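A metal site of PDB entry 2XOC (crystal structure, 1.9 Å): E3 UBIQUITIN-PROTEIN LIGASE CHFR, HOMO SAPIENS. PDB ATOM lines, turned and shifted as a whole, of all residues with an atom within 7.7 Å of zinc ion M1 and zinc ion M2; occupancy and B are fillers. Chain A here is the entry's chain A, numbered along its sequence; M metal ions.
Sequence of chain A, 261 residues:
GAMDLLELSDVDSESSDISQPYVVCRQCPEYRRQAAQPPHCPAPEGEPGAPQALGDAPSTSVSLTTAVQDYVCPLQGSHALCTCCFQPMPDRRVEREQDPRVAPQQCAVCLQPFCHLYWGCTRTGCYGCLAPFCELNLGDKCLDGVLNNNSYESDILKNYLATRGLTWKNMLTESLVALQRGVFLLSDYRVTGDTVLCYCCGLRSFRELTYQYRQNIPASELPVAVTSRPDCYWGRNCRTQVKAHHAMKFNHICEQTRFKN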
ATOM      1  N   ARG A  26      -8.683 -26.842  -4.486  1.00  0.00           N
ATOM      2  CA  ARG A  26      -8.832 -28.286  -4.666  1.00  0.00           C
ATOM      3  C   ARG A  26      -7.661 -28.918  -5.416  1.00  0.00           C
ATOM      4  O   ARG A  26      -7.267 -30.041  -5.123  1.00  0.00           O
ATOM      5  CB  ARG A  26     -10.131 -28.597  -5.423  1.00  0.00           C
ATOM      6  CG  ARG A  26     -11.361 -28.738  -4.547  1.00  0.00           C
ATOM      7  CD  ARG A  26     -12.549 -29.210  -5.386  1.00  0.00           C
ATOM      8  NE  ARG A  26     -13.720 -28.357  -5.182  1.00  0.00           N
ATOM      9  CZ  ARG A  26     -14.868 -28.481  -5.858  1.00  0.00           C
ATOM     10  NH1 ARG A  26     -14.994 -29.431  -6.769  1.00  0.00           N
ATOM     11  NH2 ARG A  26     -15.878 -27.658  -5.614  1.00  0.00           N
ATOM     12  N   LEU A  81     -12.016 -16.748  -7.924  1.00  0.00           N
ATOM     13  CA  LEU A  81     -13.046 -17.165  -6.976  1.00  0.00           C
ATOM     14  C   LEU A  81     -14.365 -17.387  -7.688  1.00  0.00           C
ATOM     15  O   LEU A  81     -14.832 -16.527  -8.438  1.00  0.00           O
ATOM     16  CB  LEU A  81     -13.219 -16.130  -5.874  1.00  0.00           C
ATOM     17  CG  LEU A  81     -12.025 -15.856  -4.959  1.00  0.00           C
ATOM     18  CD1 LEU A  81     -12.448 -14.973  -3.788  1.00  0.00           C
ATOM     19  CD2 LEU A  81     -11.427 -17.157  -4.460  1.00  0.00           C
ATOM     20  N   CYS A  82     -14.991 -18.535  -7.457  1.00  0.00           N
ATOM     21  CA  CYS A  82     -16.313 -18.790  -8.000  1.00  0.00           C
ATOM     22  C   CYS A  82     -17.287 -17.748  -7.467  1.00  0.00           C
ATOM     23  O   CYS A  82     -17.324 -17.490  -6.267  1.00  0.00           O
ATOM     24  CB  CYS A  82     -16.795 -20.193  -7.641  1.00  0.00           C
ATOM     25  SG  CYS A  82     -18.481 -20.539  -8.206  1.00  0.00           S
ATOM     26  N   THR A  83     -18.062 -17.157  -8.373  1.00  0.00           N
ATOM     27  CA  THR A  83     -18.988 -16.106  -7.994  1.00  0.00           C
ATOM     28  C   THR A  83     -20.106 -16.646  -7.106  1.00  0.00           C
ATOM     29  O   THR A  83     -20.706 -15.910  -6.324  1.00  0.00           O
ATOM     30  CB  THR A  83     -19.565 -15.423  -9.243  1.00  0.00           C
ATOM     31  OG1 THR A  83     -18.499 -14.876 -10.026  1.00  0.00           O
ATOM     32  CG2 THR A  83     -20.531 -14.306  -8.859  1.00  0.00           C
ATOM     33  N   CYS A  84     -20.364 -17.942  -7.223  1.00  0.00           N
ATOM     34  CA  CYS A  84     -21.430 -18.580  -6.460  1.00  0.00           C
ATOM     35  C   CYS A  84     -20.985 -19.025  -5.065  1.00  0.00           C
ATOM     36  O   CYS A  84     -21.544 -18.596  -4.053  1.00  0.00           O
ATOM     37  CB  CYS A  84     -22.009 -19.767  -7.235  1.00  0.00           C
ATOM     38  SG  CYS A  84     -23.107 -20.830  -6.282  1.00  0.00           S
ATOM     39  N   CYS A  85     -19.972 -19.886  -5.006  1.00  0.00           N
ATOM     40  CA  CYS A  85     -19.562 -20.485  -3.739  1.00  0.00           C
ATOM     41  C   CYS A  85     -18.365 -19.791  -3.094  1.00  0.00           C
ATOM     42  O   CYS A  85     -17.998 -20.094  -1.962  1.00  0.00           O
ATOM     43  CB  CYS A  85     -19.252 -21.975  -3.936  1.00  0.00           C
ATOM     44  SG  CYS A  85     -17.729 -22.285  -4.851  1.00  0.00           S
ATOM     45  N   PHE A  86     -17.749 -18.865  -3.826  1.00  0.00           N
ATOM     46  CA  PHE A  86     -16.624 -18.074  -3.315  1.00  0.00           C
ATOM     47  C   PHE A  86     -15.324 -18.866  -3.119  1.00  0.00           C
ATOM     48  O   PHE A  86     -14.357 -18.338  -2.578  1.00  0.00           O
ATOM     49  CB  PHE A  86     -16.987 -17.374  -2.002  1.00  0.00           C
ATOM     50  CG  PHE A  86     -18.345 -16.743  -2.002  1.00  0.00           C
ATOM     51  CD1 PHE A  86     -18.635 -15.668  -2.822  1.00  0.00           C
ATOM     52  CD2 PHE A  86     -19.340 -17.221  -1.156  1.00  0.00           C
ATOM     53  CE1 PHE A  86     -19.882 -15.085  -2.817  1.00  0.00           C
ATOM     54  CE2 PHE A  86     -20.592 -16.650  -1.148  1.00  0.00           C
ATOM     55  CZ  PHE A  86     -20.869 -15.574  -1.974  1.00  0.00           C
ATOM     56  N   GLN A  87     -15.304 -20.116  -3.556  1.00  0.00           N
ATOM     57  CA  GLN A  87     -14.109 -20.939  -3.424  1.00  0.00           C
ATOM     58  C   GLN A  87     -13.176 -20.745  -4.619  1.00  0.00           C
ATOM     59  O   GLN A  87     -13.639 -20.533  -5.742  1.00  0.00           O
ATOM     60  CB  GLN A  87     -14.469 -22.414  -3.260  1.00  0.00           C
ATOM     61  CG  GLN A  87     -15.405 -22.690  -2.090  1.00  0.00           C
ATOM     62  CD  GLN A  87     -14.925 -22.048  -0.799  1.00  0.00           C
ATOM     63  OE1 GLN A  87     -13.932 -22.472  -0.209  1.00  0.00           O
ATOM     64  NE2 GLN A  87     -15.624 -21.005  -0.361  1.00  0.00           N
ATOM     65  N   PRO A  88     -11.858 -20.813  -4.384  1.00  0.00           N
ATOM     66  CA  PRO A  88     -10.890 -20.568  -5.453  1.00  0.00           C
ATOM     67  C   PRO A  88     -10.758 -21.772  -6.395  1.00  0.00           C
ATOM     68  O   PRO A  88     -10.866 -22.923  -5.972  1.00  0.00           O
ATOM     69  CB  PRO A  88      -9.582 -20.354  -4.693  1.00  0.00           C
ATOM     70  CG  PRO A  88      -9.738 -21.197  -3.476  1.00  0.00           C
ATOM     71  CD  PRO A  88     -11.202 -21.099  -3.100  1.00  0.00           C
ATOM     72  N   MET A  89     -10.542 -21.470  -7.667  1.00  0.00           N
ATOM     73  CA  MET A  89     -10.234 -22.487  -8.665  1.00  0.00           C
ATOM     74  C   MET A  89      -9.101 -21.936  -9.510  1.00  0.00           C
ATOM     75  O   MET A  89      -8.906 -20.719  -9.562  1.00  0.00           O
ATOM     76  CB  MET A  89     -11.448 -22.774  -9.535  1.00  0.00           C
ATOM     77  CG  MET A  89     -11.957 -21.557 -10.284  1.00  0.00           C
ATOM     78  SD  MET A  89     -13.446 -21.877 -11.248  1.00  0.00           S
ATOM     79  CE  MET A  89     -13.794 -20.242 -11.882  1.00  0.00           C
ATOM     80  N   PRO A 113     -16.822 -15.442 -13.175  1.00  0.00           N
ATOM     81  CA  PRO A 113     -16.344 -16.828 -13.058  1.00  0.00           C
ATOM     82  C   PRO A 113     -17.249 -17.711 -12.198  1.00  0.00           C
ATOM     83  O   PRO A 113     -17.726 -17.249 -11.163  1.00  0.00           O
ATOM     84  CB  PRO A 113     -14.982 -16.656 -12.384  1.00  0.00           C
ATOM     85  CG  PRO A 113     -15.102 -15.410 -11.584  1.00  0.00           C
ATOM     86  CD  PRO A 113     -16.068 -14.511 -12.327  1.00  0.00           C
ATOM     87  N   PHE A 114     -17.467 -18.945 -12.642  1.00  0.00           N
ATOM     88  CA  PHE A 114     -18.222 -19.945 -11.873  1.00  0.00           C
ATOM     89  C   PHE A 114     -17.509 -21.292 -12.010  1.00  0.00           C
ATOM     90  O   PHE A 114     -16.946 -21.582 -13.062  1.00  0.00           O
ATOM     91  CB  PHE A 114     -19.655 -20.057 -12.377  1.00  0.00           C
ATOM     92  CG  PHE A 114     -20.494 -18.818 -12.151  1.00  0.00           C
ATOM     93  CD1 PHE A 114     -21.244 -18.677 -11.004  1.00  0.00           C
ATOM     94  CD2 PHE A 114     -20.498 -17.807 -13.091  1.00  0.00           C
ATOM     95  CE1 PHE A 114     -22.005 -17.537 -10.794  1.00  0.00           C
ATOM     96  CE2 PHE A 114     -21.254 -16.655 -12.885  1.00  0.00           C
ATOM     97  CZ  PHE A 114     -22.010 -16.527 -11.735  1.00  0.00           C
ATOM     98  N   CYS A 115     -17.539 -22.106 -10.957  1.00  0.00           N
ATOM     99  CA  CYS A 115     -16.718 -23.317 -10.938  1.00  0.00           C
ATOM    100  C   CYS A 115     -17.435 -24.610 -11.313  1.00  0.00           C
ATOM    101  O   CYS A 115     -16.820 -25.664 -11.387  1.00  0.00           O
ATOM    102  CB  CYS A 115     -16.063 -23.494  -9.555  1.00  0.00           C
ATOM    103  SG  CYS A 115     -17.147 -24.257  -8.316  1.00  0.00           S
ATOM    104  N   HIS A 116     -18.747 -24.529 -11.552  1.00  0.00           N
ATOM    105  CA  HIS A 116     -19.549 -25.746 -11.671  1.00  0.00           C
ATOM    106  C   HIS A 116     -19.131 -26.694 -12.787  1.00  0.00           C
ATOM    107  O   HIS A 116     -18.931 -27.881 -12.561  1.00  0.00           O
ATOM    108  CB  HIS A 116     -21.038 -25.448 -11.771  1.00  0.00           C
ATOM    109  CG  HIS A 116     -21.896 -26.664 -11.630  1.00  0.00           C
ATOM    110  ND1 HIS A 116     -21.885 -27.448 -10.501  1.00  0.00           N
ATOM    111  CD2 HIS A 116     -22.784 -27.245 -12.480  1.00  0.00           C
ATOM    112  CE1 HIS A 116     -22.729 -28.456 -10.648  1.00  0.00           C
ATOM    113  NE2 HIS A 116     -23.285 -28.352 -11.841  1.00  0.00           N
ATOM    114  N   TRP A 119     -15.315 -28.250 -12.103  1.00  0.00           N
ATOM    115  CA  TRP A 119     -15.123 -29.352 -11.165  1.00  0.00           C
ATOM    116  C   TRP A 119     -16.294 -29.613 -10.217  1.00  0.00           C
ATOM    117  O   TRP A 119     -16.157 -30.369  -9.253  1.00  0.00           O
ATOM    118  CB  TRP A 119     -13.820 -29.190 -10.369  1.00  0.00           C
ATOM    119  CG  TRP A 119     -13.756 -27.976  -9.487  1.00  0.00           C
ATOM    120  CD1 TRP A 119     -14.793 -27.224  -9.045  1.00  0.00           C
ATOM    121  CD2 TRP A 119     -12.570 -27.404  -8.918  1.00  0.00           C
ATOM    122  NE1 TRP A 119     -14.330 -26.202  -8.249  1.00  0.00           N
ATOM    123  CE2 TRP A 119     -12.973 -26.294  -8.155  1.00  0.00           C
ATOM    124  CE3 TRP A 119     -11.208 -27.708  -9.000  1.00  0.00           C
ATOM    125  CZ2 TRP A 119     -12.063 -25.489  -7.467  1.00  0.00           C
ATOM    126  CZ3 TRP A 119     -10.304 -26.916  -8.309  1.00  0.00           C
ATOM    127  CH2 TRP A 119     -10.731 -25.821  -7.555  1.00  0.00           C
ATOM    128  N   GLY A 120     -17.434 -29.001 -10.492  1.00  0.00           N
ATOM    129  CA  GLY A 120     -18.622 -29.214  -9.683  1.00  0.00           C
ATOM    130  C   GLY A 120     -18.679 -28.322  -8.461  1.00  0.00           C
ATOM    131  O   GLY A 120     -17.853 -28.425  -7.558  1.00  0.00           O
ATOM    132  N   CYS A 121     -19.683 -27.445  -8.432  1.00  0.00           N
ATOM    133  CA  CYS A 121     -19.845 -26.504  -7.341  1.00  0.00           C
ATOM    134  C   CYS A 121     -20.803 -27.080  -6.294  1.00  0.00           C
ATOM    135  O   CYS A 121     -21.725 -27.821  -6.636  1.00  0.00           O
ATOM    136  CB  CYS A 121     -20.393 -25.179  -7.885  1.00  0.00           C
ATOM    137  SG  CYS A 121     -20.600 -23.873  -6.656  1.00  0.00           S
ATOM    138  N   THR A 122     -20.574 -26.736  -5.030  1.00  0.00           N
ATOM    139  CA  THR A 122     -21.459 -27.182  -3.962  1.00  0.00           C
ATOM    140  C   THR A 122     -21.754 -26.050  -2.987  1.00  0.00           C
ATOM    141  O   THR A 122     -20.859 -25.478  -2.385  1.00  0.00           O
ATOM    142  CB  THR A 122     -20.857 -28.370  -3.181  1.00  0.00           C
ATOM    143  OG1 THR A 122     -20.651 -29.483  -4.069  1.00  0.00           O
ATOM    144  CG2 THR A 122     -21.793 -28.799  -2.064  1.00  0.00           C
ATOM    145  N   ARG A 123     -23.043 -25.730  -2.865  1.00  0.00           N
ATOM    146  CA  ARG A 123     -23.495 -24.730  -1.912  1.00  0.00           C
ATOM    147  C   ARG A 123     -24.995 -24.830  -1.758  1.00  0.00           C
ATOM    148  O   ARG A 123     -25.704 -25.107  -2.733  1.00  0.00           O
ATOM    149  CB  ARG A 123     -23.107 -23.309  -2.378  1.00  0.00           C
ATOM    150  CG  ARG A 123     -23.580 -22.214  -1.422  1.00  0.00           C
ATOM    151  CD  ARG A 123     -23.237 -20.814  -1.933  1.00  0.00           C
ATOM    152  NE  ARG A 123     -23.996 -20.466  -3.133  1.00  0.00           N
ATOM    153  CZ  ARG A 123     -25.225 -19.958  -3.118  1.00  0.00           C
ATOM    154  NH1 ARG A 123     -25.851 -19.744  -1.965  1.00  0.00           N
ATOM    155  NH2 ARG A 123     -25.831 -19.656  -4.261  1.00  0.00           N
ATOM    156  N   GLY A 125     -28.361 -23.572  -2.006  1.00  0.00           N
ATOM    157  CA  GLY A 125     -28.864 -22.496  -2.848  1.00  0.00           C
ATOM    158  C   GLY A 125     -28.308 -22.607  -4.251  1.00  0.00           C
ATOM    159  O   GLY A 125     -28.878 -22.052  -5.200  1.00  0.00           O
ATOM    160  N   CYS A 126     -27.187 -23.308  -4.395  1.00  0.00           N
ATOM    161  CA  CYS A 126     -26.636 -23.581  -5.720  1.00  0.00           C
ATOM    162  C   CYS A 126     -27.293 -24.817  -6.329  1.00  0.00           C
ATOM    163  O   CYS A 126     -27.275 -25.892  -5.735  1.00  0.00           O
ATOM    164  CB  CYS A 126     -25.113 -23.762  -5.670  1.00  0.00           C
ATOM    165  SG  CYS A 126     -24.399 -24.257  -7.258  1.00  0.00           S
ATOM    166  N   TYR A 127     -27.865 -24.648  -7.514  1.00  0.00           N
ATOM    167  CA  TYR A 127     -28.528 -25.743  -8.209  1.00  0.00           C
ATOM    168  C   TYR A 127     -27.624 -26.316  -9.302  1.00  0.00           C
ATOM    169  O   TYR A 127     -28.015 -27.248 -10.006  1.00  0.00           O
ATOM    170  CB  TYR A 127     -29.821 -25.253  -8.883  1.00  0.00           C
ATOM    171  CG  TYR A 127     -30.770 -24.483  -7.993  1.00  0.00           C
ATOM    172  CD1 TYR A 127     -31.199 -24.993  -6.768  1.00  0.00           C
ATOM    173  CD2 TYR A 127     -31.272 -23.241  -8.389  1.00  0.00           C
ATOM    174  CE1 TYR A 127     -32.069 -24.284  -5.966  1.00  0.00           C
ATOM    175  CE2 TYR A 127     -32.142 -22.532  -7.587  1.00  0.00           C
ATOM    176  CZ  TYR A 127     -32.545 -23.056  -6.376  1.00  0.00           C
ATOM    177  OH  TYR A 127     -33.419 -22.356  -5.584  1.00  0.00           O
ATOM    178  N   GLY A 128     -26.425 -25.771  -9.419  1.00  0.00           N
ATOM    179  CA  GLY A 128     -25.567 -26.014 -10.563  1.00  0.00           C
ATOM    180  C   GLY A 128     -25.465 -24.707 -11.337  1.00  0.00           C
ATOM    181  O   GLY A 128     -26.237 -24.476 -12.268  1.00  0.00           O
ATOM    182  N   CYS A 129     -24.523 -23.869 -10.940  1.00  0.00           N
ATOM    183  CA  CYS A 129     -24.541 -22.443 -11.258  1.00  0.00           C
ATOM    184  C   CYS A 129     -24.049 -22.068 -12.647  1.00  0.00           C
ATOM    185  O   CYS A 129     -24.119 -20.902 -13.037  1.00  0.00           O
ATOM    186  CB  CYS A 129     -23.761 -21.666 -10.189  1.00  0.00           C
ATOM    187  SG  CYS A 129     -22.099 -22.333  -9.886  1.00  0.00           S
ATOM    188  N   LEU A 130     -23.558 -23.042 -13.407  1.00  0.00           N
ATOM    189  CA  LEU A 130     -23.127 -22.778 -14.780  1.00  0.00           C
ATOM    190  C   LEU A 130     -23.488 -23.942 -15.698  1.00  0.00           C
ATOM    191  O   LEU A 130     -23.167 -25.087 -15.401  1.00  0.00           O
ATOM    192  CB  LEU A 130     -21.617 -22.540 -14.816  1.00  0.00           C
ATOM    193  CG  LEU A 130     -21.016 -22.063 -16.133  1.00  0.00           C
ATOM    194  CD1 LEU A 130     -21.540 -20.678 -16.498  1.00  0.00           C
ATOM    195  CD2 LEU A 130     -19.496 -22.071 -16.054  1.00  0.00           C
ATOM    196  N   TYR A 199     -26.621 -19.135 -13.290  1.00  0.00           N
ATOM    197  CA  TYR A 199     -27.964 -19.178 -12.741  1.00  0.00           C
ATOM    198  C   TYR A 199     -28.720 -17.858 -12.888  1.00  0.00           C
ATOM    199  O   TYR A 199     -29.840 -17.841 -13.397  1.00  0.00           O
ATOM    200  CB  TYR A 199     -27.930 -19.592 -11.266  1.00  0.00           C
ATOM    201  CG  TYR A 199     -29.219 -19.299 -10.539  1.00  0.00           C
ATOM    202  CD1 TYR A 199     -30.327 -20.117 -10.705  1.00  0.00           C
ATOM    203  CD2 TYR A 199     -29.322 -18.202  -9.706  1.00  0.00           C
ATOM    204  CE1 TYR A 199     -31.512 -19.837 -10.047  1.00  0.00           C
ATOM    205  CE2 TYR A 199     -30.507 -17.922  -9.048  1.00  0.00           C
ATOM    206  CZ  TYR A 199     -31.589 -18.738  -9.223  1.00  0.00           C
ATOM    207  OH  TYR A 199     -32.763 -18.461  -8.557  1.00  0.00           O
HETATM  208 ZN    ZN M   1     -18.514 -22.669  -7.135  1.00  0.00          ZN
HETATM  209 ZN    ZN M   2     -22.550 -22.761  -7.519  1.00  0.00          ZN
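Along chain A the residues within 4 Å of zinc ion M1 span positions 82 to 121.
The nearest printed residue that does not touch zinc ion M1 is Cys 129 (4.5 Å).
Zinc ion M1 is bound by the side-chain sulfur of Cys 82 (2.4 Å), the side-chain sulfur of Cys 115 (2.4 Å), the side-chain sulfur of Cys 85 (2.4 Å) and the side-chain sulfur of Cys 121 (2.5 Å).
Zinc ion M2 is bound by SG of Cys 84 (2.4 Å).
SG of Cys 126 binds zinc ion M2 (2.4 Å).
Zinc ion M2 is bound by SG of Cys 121 (2.4 Å).
Zinc ion M2 is bound by the side-chain sulfur (SG) of Cys 129 (2.4 Å).
Within 4 Å of zinc ion M2: Cys 84, Cys 121, Cys 126 and Cys 129.
The backbone NH of Cys 84 sits close to the side-chain sulfur of Cys 82, 3.4 Å away.
The guanidinium group (NE) of Arg 123 lies within hydrogen-bond range of the backbone carbonyl oxygen (O) of Cys 84 (3.2 Å).
N of Cys 82 sits at hydrogen-bond distance from O of Gln 87 (3.0 Å).
SG of Cys 126 sits close to N of Gly 128.
A ring nitrogen (ND1) of His 116 lies within hydrogen-bond range of the backbone NH (N) of Cys 121.
SG of Cys 115 lies close to NE1 of Trp 119, 3.4 Å away.
The backbone carbonyl oxygen (O) of Cys 85 lies within hydrogen-bond range of the side-chain amide nitrogen (NE2) of Gln 87, 3.0 Å away.
O of Cys 129 sits at hydrogen-bond distance from N of Tyr 199 (3.1 Å).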
